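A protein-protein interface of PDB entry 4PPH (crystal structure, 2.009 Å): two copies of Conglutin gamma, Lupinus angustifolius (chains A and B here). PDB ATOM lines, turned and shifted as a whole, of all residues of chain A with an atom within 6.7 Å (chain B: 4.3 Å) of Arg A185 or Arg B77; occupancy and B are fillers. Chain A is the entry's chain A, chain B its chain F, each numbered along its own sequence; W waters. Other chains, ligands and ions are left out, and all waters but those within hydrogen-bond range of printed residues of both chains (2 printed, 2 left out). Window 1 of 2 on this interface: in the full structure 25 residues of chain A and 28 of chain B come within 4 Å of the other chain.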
ATOM      1  N   GLN A 168      19.511 -32.652  25.433  1.00  0.00           N
ATOM      2  CA  GLN A 168      19.092 -31.765  24.351  1.00  0.00           C
ATOM      3  C   GLN A 168      18.079 -30.728  24.850  1.00  0.00           C
ATOM      4  O   GLN A 168      16.879 -30.932  24.782  1.00  0.00           O
ATOM      5  CB  GLN A 168      18.475 -32.589  23.231  1.00  0.00           C
ATOM      6  CG  GLN A 168      19.469 -33.356  22.489  1.00  0.00           C
ATOM      7  CD  GLN A 168      20.412 -32.440  21.815  1.00  0.00           C
ATOM      8  OE1 GLN A 168      20.023 -31.696  20.915  1.00  0.00           O
ATOM      9  NE2 GLN A 168      21.665 -32.434  22.269  1.00  0.00           N
ATOM     10  N   GLN A 174      26.582 -28.571  27.329  1.00  0.00           N
ATOM     11  CA  GLN A 174      27.261 -28.562  26.030  1.00  0.00           C
ATOM     12  C   GLN A 174      26.716 -27.439  25.143  1.00  0.00           C
ATOM     13  O   GLN A 174      27.471 -26.804  24.415  1.00  0.00           O
ATOM     14  CB  GLN A 174      27.172 -29.942  25.330  1.00  0.00           C
ATOM     15  CG  GLN A 174      25.904 -30.265  24.549  1.00  0.00           C
ATOM     16  CD  GLN A 174      24.778 -30.706  25.435  1.00  0.00           C
ATOM     17  OE1 GLN A 174      24.946 -30.829  26.639  1.00  0.00           O
ATOM     18  NE2 GLN A 174      23.619 -30.942  24.847  1.00  0.00           N
ATOM     19  N   ASN A 175      25.421 -27.173  25.227  1.00  0.00           N
ATOM     20  CA  ASN A 175      24.802 -26.129  24.418  1.00  0.00           C
ATOM     21  C   ASN A 175      25.418 -24.761  24.746  1.00  0.00           C
ATOM     22  O   ASN A 175      25.683 -23.962  23.847  1.00  0.00           O
ATOM     23  CB  ASN A 175      23.283 -26.089  24.668  1.00  0.00           C
ATOM     24  CG  ASN A 175      22.567 -24.926  23.937  1.00  0.00           C
ATOM     25  OD1 ASN A 175      22.762 -23.747  24.252  1.00  0.00           O
ATOM     26  ND2 ASN A 175      21.704 -25.272  22.988  1.00  0.00           N
ATOM     27  N   GLN A 176      25.715 -24.520  26.025  1.00  0.00           N
ATOM     28  CA  GLN A 176      26.320 -23.259  26.450  1.00  0.00           C
ATOM     29  C   GLN A 176      27.815 -23.164  26.111  1.00  0.00           C
ATOM     30  O   GLN A 176      28.296 -22.085  25.769  1.00  0.00           O
ATOM     31  CB  GLN A 176      26.104 -23.043  27.949  1.00  0.00           C
ATOM     32  CG  GLN A 176      24.643 -22.719  28.322  1.00  0.00           C
ATOM     33  CD  GLN A 176      24.472 -22.222  29.754  1.00  0.00           C
ATOM     34  OE1 GLN A 176      24.804 -21.087  30.065  1.00  0.00           O
ATOM     35  NE2 GLN A 176      23.967 -23.077  30.624  1.00  0.00           N
ATOM     36  N   PHE A 178      29.234 -24.871  23.496  1.00  0.00           N
ATOM     37  CA  PHE A 178      29.255 -24.738  22.031  1.00  0.00           C
ATOM     38  C   PHE A 178      29.149 -23.292  21.617  1.00  0.00           C
ATOM     39  O   PHE A 178      29.893 -22.794  20.774  1.00  0.00           O
ATOM     40  CB  PHE A 178      28.101 -25.481  21.368  1.00  0.00           C
ATOM     41  CG  PHE A 178      28.156 -26.962  21.509  1.00  0.00           C
ATOM     42  CD1 PHE A 178      29.337 -27.607  21.834  1.00  0.00           C
ATOM     43  CD2 PHE A 178      27.036 -27.717  21.274  1.00  0.00           C
ATOM     44  CE1 PHE A 178      29.383 -28.976  21.958  1.00  0.00           C
ATOM     45  CE2 PHE A 178      27.073 -29.096  21.377  1.00  0.00           C
ATOM     46  CZ  PHE A 178      28.255 -29.729  21.723  1.00  0.00           C
ATOM     47  N   SER A 179      28.174 -22.624  22.207  1.00  0.00           N
ATOM     48  CA  SER A 179      27.813 -21.314  21.744  1.00  0.00           C
ATOM     49  C   SER A 179      28.791 -20.261  22.183  1.00  0.00           C
ATOM     50  O   SER A 179      29.109 -19.348  21.437  1.00  0.00           O
ATOM     51  CB  SER A 179      26.390 -20.980  22.226  1.00  0.00           C
ATOM     52  OG  SER A 179      26.333 -20.688  23.613  1.00  0.00           O
ATOM     53  N   LEU A 183      32.196 -23.730  19.080  1.00  0.00           N
ATOM     54  CA  LEU A 183      32.638 -25.107  18.828  1.00  0.00           C
ATOM     55  C   LEU A 183      31.768 -25.842  17.820  1.00  0.00           C
ATOM     56  O   LEU A 183      30.619 -25.480  17.636  1.00  0.00           O
ATOM     57  CB  LEU A 183      32.633 -25.899  20.129  1.00  0.00           C
ATOM     58  CG  LEU A 183      33.416 -25.299  21.300  1.00  0.00           C
ATOM     59  CD1 LEU A 183      33.168 -26.166  22.521  1.00  0.00           C
ATOM     60  CD2 LEU A 183      34.890 -25.209  20.976  1.00  0.00           C
ATOM     61  N   LYS A 184      32.309 -26.880  17.184  1.00  0.00           N
ATOM     62  CA  LYS A 184      31.490 -27.825  16.413  1.00  0.00           C
ATOM     63  C   LYS A 184      30.525 -28.502  17.385  1.00  0.00           C
ATOM     64  O   LYS A 184      30.917 -28.746  18.513  1.00  0.00           O
ATOM     65  CB  LYS A 184      32.369 -28.845  15.683  1.00  0.00           C
ATOM     66  CG  LYS A 184      31.601 -30.024  15.104  1.00  0.00           C
ATOM     67  CD  LYS A 184      32.386 -30.754  14.042  1.00  0.00           C
ATOM     68  CE  LYS A 184      31.662 -31.993  13.501  1.00  0.00           C
ATOM     69  NZ  LYS A 184      30.230 -32.119  13.889  1.00  0.00           N
ATOM     70  N   ARG A 185      29.270 -28.759  16.977  1.00  0.00           N
ATOM     71  CA  ARG A 185      28.241 -29.355  17.853  1.00  0.00           C
ATOM     72  C   ARG A 185      28.368 -30.884  17.941  1.00  0.00           C
ATOM     73  O   ARG A 185      27.688 -31.640  17.239  1.00  0.00           O
ATOM     74  CB  ARG A 185      26.837 -28.952  17.390  1.00  0.00           C
ATOM     75  CG  ARG A 185      26.648 -27.420  17.330  1.00  0.00           C
ATOM     76  CD  ARG A 185      25.209 -26.993  17.029  1.00  0.00           C
ATOM     77  NE  ARG A 185      24.329 -27.188  18.172  1.00  0.00           N
ATOM     78  CZ  ARG A 185      24.163 -26.292  19.141  1.00  0.00           C
ATOM     79  NH1 ARG A 185      23.353 -26.558  20.151  1.00  0.00           N
ATOM     80  NH2 ARG A 185      24.799 -25.129  19.099  1.00  0.00           N
ATOM     81  N   GLN A 186      29.257 -31.302  18.837  1.00  0.00           N
ATOM     82  CA  GLN A 186      29.638 -32.686  19.021  1.00  0.00           C
ATOM     83  C   GLN A 186      30.257 -32.829  20.394  1.00  0.00           C
ATOM     84  O   GLN A 186      30.986 -31.947  20.825  1.00  0.00           O
ATOM     85  CB  GLN A 186      30.610 -33.074  17.933  1.00  0.00           C
ATOM     86  CG  GLN A 186      31.132 -34.461  17.913  1.00  0.00           C
ATOM     87  CD  GLN A 186      32.311 -34.541  16.981  1.00  0.00           C
ATOM     88  OE1 GLN A 186      33.441 -34.594  17.420  1.00  0.00           O
ATOM     89  NE2 GLN A 186      32.058 -34.482  15.688  1.00  0.00           N
ATOM     90  N   PHE A 187      29.930 -33.890  21.124  1.00  0.00           N
ATOM     91  CA  PHE A 187      30.695 -34.203  22.326  1.00  0.00           C
ATOM     92  C   PHE A 187      30.918 -35.698  22.408  1.00  0.00           C
ATOM     93  O   PHE A 187      30.134 -36.464  21.896  1.00  0.00           O
ATOM     94  CB  PHE A 187      30.019 -33.659  23.600  1.00  0.00           C
ATOM     95  CG  PHE A 187      28.677 -34.296  23.947  1.00  0.00           C
ATOM     96  CD1 PHE A 187      27.491 -33.802  23.425  1.00  0.00           C
ATOM     97  CD2 PHE A 187      28.600 -35.337  24.851  1.00  0.00           C
ATOM     98  CE1 PHE A 187      26.277 -34.356  23.773  1.00  0.00           C
ATOM     99  CE2 PHE A 187      27.370 -35.881  25.196  1.00  0.00           C
ATOM    100  CZ  PHE A 187      26.221 -35.393  24.661  1.00  0.00           C
ATOM    101  N   GLY A 204      33.670 -30.387  21.261  1.00  0.00           N
ATOM    102  CA  GLY A 204      34.198 -29.832  20.041  1.00  0.00           C
ATOM    103  C   GLY A 204      34.606 -30.924  19.074  1.00  0.00           C
ATOM    104  O   GLY A 204      34.469 -32.114  19.344  1.00  0.00           O
ATOM    105  N   ASP A 205      35.140 -30.504  17.939  1.00  0.00           N
ATOM    106  CA  ASP A 205      35.477 -31.424  16.866  1.00  0.00           C
ATOM    107  C   ASP A 205      36.736 -32.231  17.153  1.00  0.00           C
ATOM    108  O   ASP A 205      37.821 -31.675  17.324  1.00  0.00           O
ATOM    109  CB  ASP A 205      35.659 -30.651  15.576  1.00  0.00           C
ATOM    110  CG  ASP A 205      35.832 -31.548  14.377  1.00  0.00           C
ATOM    111  OD1 ASP A 205      35.605 -32.784  14.470  1.00  0.00           O
ATOM    112  OD2 ASP A 205      36.180 -30.983  13.320  1.00  0.00           O
ATOM    113  N   PHE A 387      28.816 -38.216  20.356  1.00  0.00           N
ATOM    114  CA  PHE A 387      27.497 -37.711  20.073  1.00  0.00           C
ATOM    115  C   PHE A 387      27.614 -36.634  19.040  1.00  0.00           C
ATOM    116  O   PHE A 387      27.998 -35.509  19.355  1.00  0.00           O
ATOM    117  CB  PHE A 387      26.859 -37.196  21.340  1.00  0.00           C
ATOM    118  CG  PHE A 387      26.580 -38.271  22.326  1.00  0.00           C
ATOM    119  CD1 PHE A 387      27.607 -38.782  23.115  1.00  0.00           C
ATOM    120  CD2 PHE A 387      25.298 -38.778  22.470  1.00  0.00           C
ATOM    121  CE1 PHE A 387      27.367 -39.785  24.016  1.00  0.00           C
ATOM    122  CE2 PHE A 387      25.049 -39.780  23.377  1.00  0.00           C
ATOM    123  CZ  PHE A 387      26.097 -40.285  24.154  1.00  0.00           C
ATOM    124  N   ASP A 388      27.356 -37.001  17.787  1.00  0.00           N
ATOM    125  CA  ASP A 388      27.480 -36.050  16.697  1.00  0.00           C
ATOM    126  C   ASP A 388      26.135 -35.367  16.456  1.00  0.00           C
ATOM    127  O   ASP A 388      25.343 -35.841  15.646  1.00  0.00           O
ATOM    128  CB  ASP A 388      27.972 -36.757  15.440  1.00  0.00           C
ATOM    129  CG  ASP A 388      28.343 -35.792  14.329  1.00  0.00           C
ATOM    130  OD1 ASP A 388      28.040 -34.582  14.438  1.00  0.00           O
ATOM    131  OD2 ASP A 388      28.966 -36.237  13.343  1.00  0.00           O
ATOM    132  N   LEU A 389      25.910 -34.231  17.123  1.00  0.00           N
ATOM    133  CA  LEU A 389      24.628 -33.566  17.096  1.00  0.00           C
ATOM    134  C   LEU A 389      24.406 -32.899  15.765  1.00  0.00           C
ATOM    135  O   LEU A 389      23.279 -32.678  15.345  1.00  0.00           O
ATOM    136  CB  LEU A 389      24.546 -32.541  18.215  1.00  0.00           C
ATOM    137  CG  LEU A 389      24.988 -33.168  19.528  1.00  0.00           C
ATOM    138  CD1 LEU A 389      25.216 -32.098  20.529  1.00  0.00           C
ATOM    139  CD2 LEU A 389      23.900 -34.112  19.995  1.00  0.00           C
ATOM    140  N   GLU A 390      25.493 -32.580  15.101  1.00  0.00           N
ATOM    141  CA  GLU A 390      25.418 -31.907  13.828  1.00  0.00           C
ATOM    142  C   GLU A 390      24.903 -32.819  12.695  1.00  0.00           C
ATOM    143  O   GLU A 390      24.258 -32.354  11.749  1.00  0.00           O
ATOM    144  CB  GLU A 390      26.792 -31.335  13.533  1.00  0.00           C
ATOM    145  CG  GLU A 390      26.960 -30.735  12.200  1.00  0.00           C
ATOM    146  CD  GLU A 390      28.411 -30.538  11.898  1.00  0.00           C
ATOM    147  OE1 GLU A 390      28.888 -31.162  10.926  1.00  0.00           O
ATOM    148  OE2 GLU A 390      29.077 -29.799  12.659  1.00  0.00           O
ATOM    149  N   ARG A 391      25.163 -34.118  12.797  1.00  0.00           N
ATOM    150  CA  ARG A 391      24.664 -35.079  11.802  1.00  0.00           C
ATOM    151  C   ARG A 391      23.589 -35.984  12.409  1.00  0.00           C
ATOM    152  O   ARG A 391      23.115 -36.905  11.745  1.00  0.00           O
ATOM    153  CB  ARG A 391      25.794 -35.950  11.242  1.00  0.00           C
ATOM    154  CG  ARG A 391      26.887 -35.149  10.574  1.00  0.00           C
ATOM    155  CD  ARG A 391      27.896 -35.987   9.806  1.00  0.00           C
ATOM    156  NE  ARG A 391      27.283 -36.930   8.875  1.00  0.00           N
ATOM    157  CZ  ARG A 391      27.961 -37.628   7.959  1.00  0.00           C
ATOM    158  NH1 ARG A 391      29.283 -37.468   7.829  1.00  0.00           N
ATOM    159  NH2 ARG A 391      27.315 -38.477   7.159  1.00  0.00           N
ATOM    160  N   THR B  73      18.344 -34.510  16.092  1.00  0.00           N
ATOM    161  CA  THR B  73      18.902 -33.428  16.914  1.00  0.00           C
ATOM    162  C   THR B  73      18.593 -32.039  16.353  1.00  0.00           C
ATOM    163  O   THR B  73      18.459 -31.078  17.099  1.00  0.00           O
ATOM    164  CB  THR B  73      20.405 -33.576  17.038  1.00  0.00           C
ATOM    165  OG1 THR B  73      20.972 -33.689  15.721  1.00  0.00           O
ATOM    166  CG2 THR B  73      20.731 -34.835  17.854  1.00  0.00           C
ATOM    167  N   GLN B  74      18.508 -31.926  15.032  1.00  0.00           N
ATOM    168  CA  GLN B  74      18.090 -30.676  14.429  1.00  0.00           C
ATOM    169  C   GLN B  74      16.646 -30.292  14.788  1.00  0.00           C
ATOM    170  O   GLN B  74      16.333 -29.133  15.088  1.00  0.00           O
ATOM    171  CB  GLN B  74      18.225 -30.753  12.909  1.00  0.00           C
ATOM    172  CG  GLN B  74      19.651 -30.859  12.432  1.00  0.00           C
ATOM    173  CD  GLN B  74      19.986 -32.235  12.060  1.00  0.00           C
ATOM    174  OE1 GLN B  74      19.427 -33.167  12.604  1.00  0.00           O
ATOM    175  NE2 GLN B  74      20.869 -32.394  11.099  1.00  0.00           N
ATOM    176  N   CYS B  75      15.766 -31.277  14.760  1.00  0.00           N
ATOM    177  CA  CYS B  75      14.387 -31.039  15.124  1.00  0.00           C
ATOM    178  C   CYS B  75      14.283 -30.711  16.600  1.00  0.00           C
ATOM    179  O   CYS B  75      13.476 -29.884  16.997  1.00  0.00           O
ATOM    180  CB  CYS B  75      13.523 -32.243  14.742  1.00  0.00           C
ATOM    181  SG  CYS B  75      13.504 -32.446  12.937  1.00  0.00           S
ATOM    182  N   SER B  76      15.107 -31.342  17.417  1.00  0.00           N
ATOM    183  CA  SER B  76      15.160 -30.988  18.838  1.00  0.00           C
ATOM    184  C   SER B  76      15.589 -29.542  19.078  1.00  0.00           C
ATOM    185  O   SER B  76      14.957 -28.825  19.840  1.00  0.00           O
ATOM    186  CB  SER B  76      16.109 -31.904  19.605  1.00  0.00           C
ATOM    187  OG  SER B  76      16.122 -31.521  20.967  1.00  0.00           O
ATOM    188  N   ARG B  77      16.661 -29.116  18.426  1.00  0.00           N
ATOM    189  CA  ARG B  77      17.139 -27.762  18.584  1.00  0.00           C
ATOM    190  C   ARG B  77      16.095 -26.744  18.151  1.00  0.00           C
ATOM    191  O   ARG B  77      15.907 -25.711  18.806  1.00  0.00           O
ATOM    192  CB  ARG B  77      18.421 -27.567  17.795  1.00  0.00           C
ATOM    193  CG  ARG B  77      19.066 -26.254  18.118  1.00  0.00           C
ATOM    194  CD  ARG B  77      20.387 -26.022  17.402  1.00  0.00           C
ATOM    195  NE  ARG B  77      20.915 -24.705  17.770  1.00  0.00           N
ATOM    196  CZ  ARG B  77      21.862 -24.058  17.097  1.00  0.00           C
ATOM    197  NH1 ARG B  77      22.259 -22.864  17.512  1.00  0.00           N
ATOM    198  NH2 ARG B  77      22.412 -24.608  16.024  1.00  0.00           N
ATOM    199  N   ALA B  78      15.377 -27.058  17.075  1.00  0.00           N
ATOM    200  CA  ALA B  78      14.365 -26.150  16.552  1.00  0.00           C
ATOM    201  C   ALA B  78      13.132 -26.157  17.401  1.00  0.00           C
ATOM    202  O   ALA B  78      12.253 -25.347  17.193  1.00  0.00           O
ATOM    203  CB  ALA B  78      13.992 -26.506  15.128  1.00  0.00           C
ATOM    204  N   ASN B  79      13.087 -27.068  18.361  1.00  0.00           N
ATOM    205  CA  ASN B  79      11.957 -27.222  19.263  1.00  0.00           C
ATOM    206  C   ASN B  79      10.686 -27.688  18.534  1.00  0.00           C
ATOM    207  O   ASN B  79       9.593 -27.210  18.799  1.00  0.00           O
ATOM    208  CB  ASN B  79      11.705 -25.905  20.009  1.00  0.00           C
ATOM    209  CG  ASN B  79      10.793 -26.073  21.193  1.00  0.00           C
ATOM    210  OD1 ASN B  79      10.726 -27.149  21.791  1.00  0.00           O
ATOM    211  ND2 ASN B  79      10.056 -25.017  21.526  1.00  0.00           N
ATOM    212  N   PRO B 170      15.106 -20.483  19.829  1.00  0.00           N
ATOM    213  CA  PRO B 170      16.323 -21.288  19.681  1.00  0.00           C
ATOM    214  C   PRO B 170      16.891 -21.317  18.285  1.00  0.00           C
ATOM    215  O   PRO B 170      18.085 -21.455  18.181  1.00  0.00           O
ATOM    216  CB  PRO B 170      15.884 -22.680  20.102  1.00  0.00           C
ATOM    217  CG  PRO B 170      14.414 -22.677  20.021  1.00  0.00           C
ATOM    218  CD  PRO B 170      14.012 -21.294  20.384  1.00  0.00           C
ATOM    219  N   ILE B 171      16.111 -21.200  17.218  1.00  0.00           N
ATOM    220  CA  ILE B 171      16.797 -21.105  15.939  1.00  0.00           C
ATOM    221  C   ILE B 171      16.589 -19.774  15.210  1.00  0.00           C
ATOM    222  O   ILE B 171      16.597 -19.711  13.983  1.00  0.00           O
ATOM    223  CB  ILE B 171      16.431 -22.275  15.021  1.00  0.00           C
ATOM    224  CG1 ILE B 171      14.932 -22.311  14.698  1.00  0.00           C
ATOM    225  CG2 ILE B 171      16.926 -23.570  15.663  1.00  0.00           C
ATOM    226  CD1 ILE B 171      14.631 -23.056  13.445  1.00  0.00           C
ATOM    227  N   ASN B 175      20.752 -16.072  17.106  1.00  0.00           N
ATOM    228  CA  ASN B 175      21.048 -17.148  18.031  1.00  0.00           C
ATOM    229  C   ASN B 175      21.983 -18.153  17.345  1.00  0.00           C
ATOM    230  O   ASN B 175      22.950 -18.620  17.952  1.00  0.00           O
ATOM    231  CB  ASN B 175      19.705 -17.759  18.476  1.00  0.00           C
ATOM    232  CG  ASN B 175      19.827 -18.862  19.504  1.00  0.00           C
ATOM    233  OD1 ASN B 175      20.126 -20.008  19.172  1.00  0.00           O
ATOM    234  ND2 ASN B 175      19.519 -18.535  20.762  1.00  0.00           N
ATOM    235  N   GLN B 176      21.735 -18.448  16.071  1.00  0.00           N
ATOM    236  CA  GLN B 176      22.582 -19.379  15.319  1.00  0.00           C
ATOM    237  C   GLN B 176      23.948 -18.758  14.922  1.00  0.00           C
ATOM    238  O   GLN B 176      24.967 -19.432  14.878  1.00  0.00           O
ATOM    239  CB  GLN B 176      21.849 -19.876  14.072  1.00  0.00           C
ATOM    240  CG  GLN B 176      20.726 -20.833  14.358  1.00  0.00           C
ATOM    241  CD  GLN B 176      20.210 -21.508  13.110  1.00  0.00           C
ATOM    242  OE1 GLN B 176      20.852 -22.394  12.563  1.00  0.00           O
ATOM    243  NE2 GLN B 176      19.045 -21.080  12.642  1.00  0.00           N
ATOM    244  N   SER B 179      26.154 -18.593  18.190  1.00  0.00           N
ATOM    245  CA  SER B 179      26.697 -19.869  18.641  1.00  0.00           C
ATOM    246  C   SER B 179      27.683 -20.470  17.636  1.00  0.00           C
ATOM    247  O   SER B 179      28.616 -21.129  18.026  1.00  0.00           O
ATOM    248  CB  SER B 179      25.570 -20.858  18.950  1.00  0.00           C
ATOM    249  OG  SER B 179      25.014 -21.393  17.773  1.00  0.00           O
HETATM  250  O   HOH W   1      21.150 -35.396   9.607  1.00  0.00           O
HETATM  251  O   HOH W   2      20.686 -30.400  18.851  1.00  0.00           O
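Of the 18 printed residues of chain A, 6 touch a printed residue of chain B.
Water W2 bridges OE1 of Gln A168 (2.5 Å) and O of Thr B73 (2.9 Å). Water W1 lies within hydrogen-bond range of O of Arg A391 (3.3 Å) and NE2 of Gln B74 (3.4 Å).
The backbone carbonyl oxygen (O) of Phe A178 lies close to the backbone carbonyl oxygen (O) of Ser B179. O of Leu A389 lies within hydrogen-bond range of OG1 of Thr B73 (2.5 Å). The backbone carbonyl oxygen (O) of Glu A390 is in hydrogen-bond range of the side-chain amide nitrogen (NE2) of Gln B74 (3.5 Å).
The backbone NH (N) of Glu A390 is in hydrogen-bond range of the backbone carbonyl oxygen (O) of Arg A185 (3.2 Å). NZ of Lys A184 lies within salt-bridge range of OE2 of Glu A390 (2.9 Å). The backbone carbonyl oxygen (O) of Gln A176 is in hydrogen-bond range of the side-chain hydroxyl (OG) of Ser A179 (3.2 Å). O of Gln B176 sits at hydrogen-bond distance from OG of Ser B179 (3.5 Å). O of Asn A175 is in hydrogen-bond range of OG of Ser A179 (3.3 Å). The backbone carbonyl oxygen of Arg A185 is in hydrogen-bond range of the backbone NH of Leu A389 (3.1 Å).
Ser B179 touches its own counterpart, Ser A179. 3 positions are printed for both chains. Of the 7 pairs that touch across the chains among the printed residues, 1 has its exchanged pair printed and touching as well.
Gln A174 touches none of the printed residues of chain B. Of chain B, only Arg B77 and Ser B179 come within 4 Å of Arg A185. Asp A388 touches none of the printed residues of chain B. Of the printed residues of chain B, Glu A390 touches Gln B74. Arg B77 touches just one residue of chain A: Arg A185 (3.7 Å). Printed residues of chain A within 4 Å of Ser B179: Phe A178, Ser A179 and Arg A185. The nearest printed residue of chain B that does not touch Arg A185 is Asn B175 (6.9 Å). The nearest residue of chain A that does not touch Arg B77 is Gln A168 (4.9 Å).
Among the printed residues, merely in contact across the chains: Gln A168 with Ser B76 (3.4 Å), Ser A179 with Ser B179 (3.4 Å), Arg A185 with Arg B77 (3.7 Å) and Arg A185 with Ser B179 (3.97 Å).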
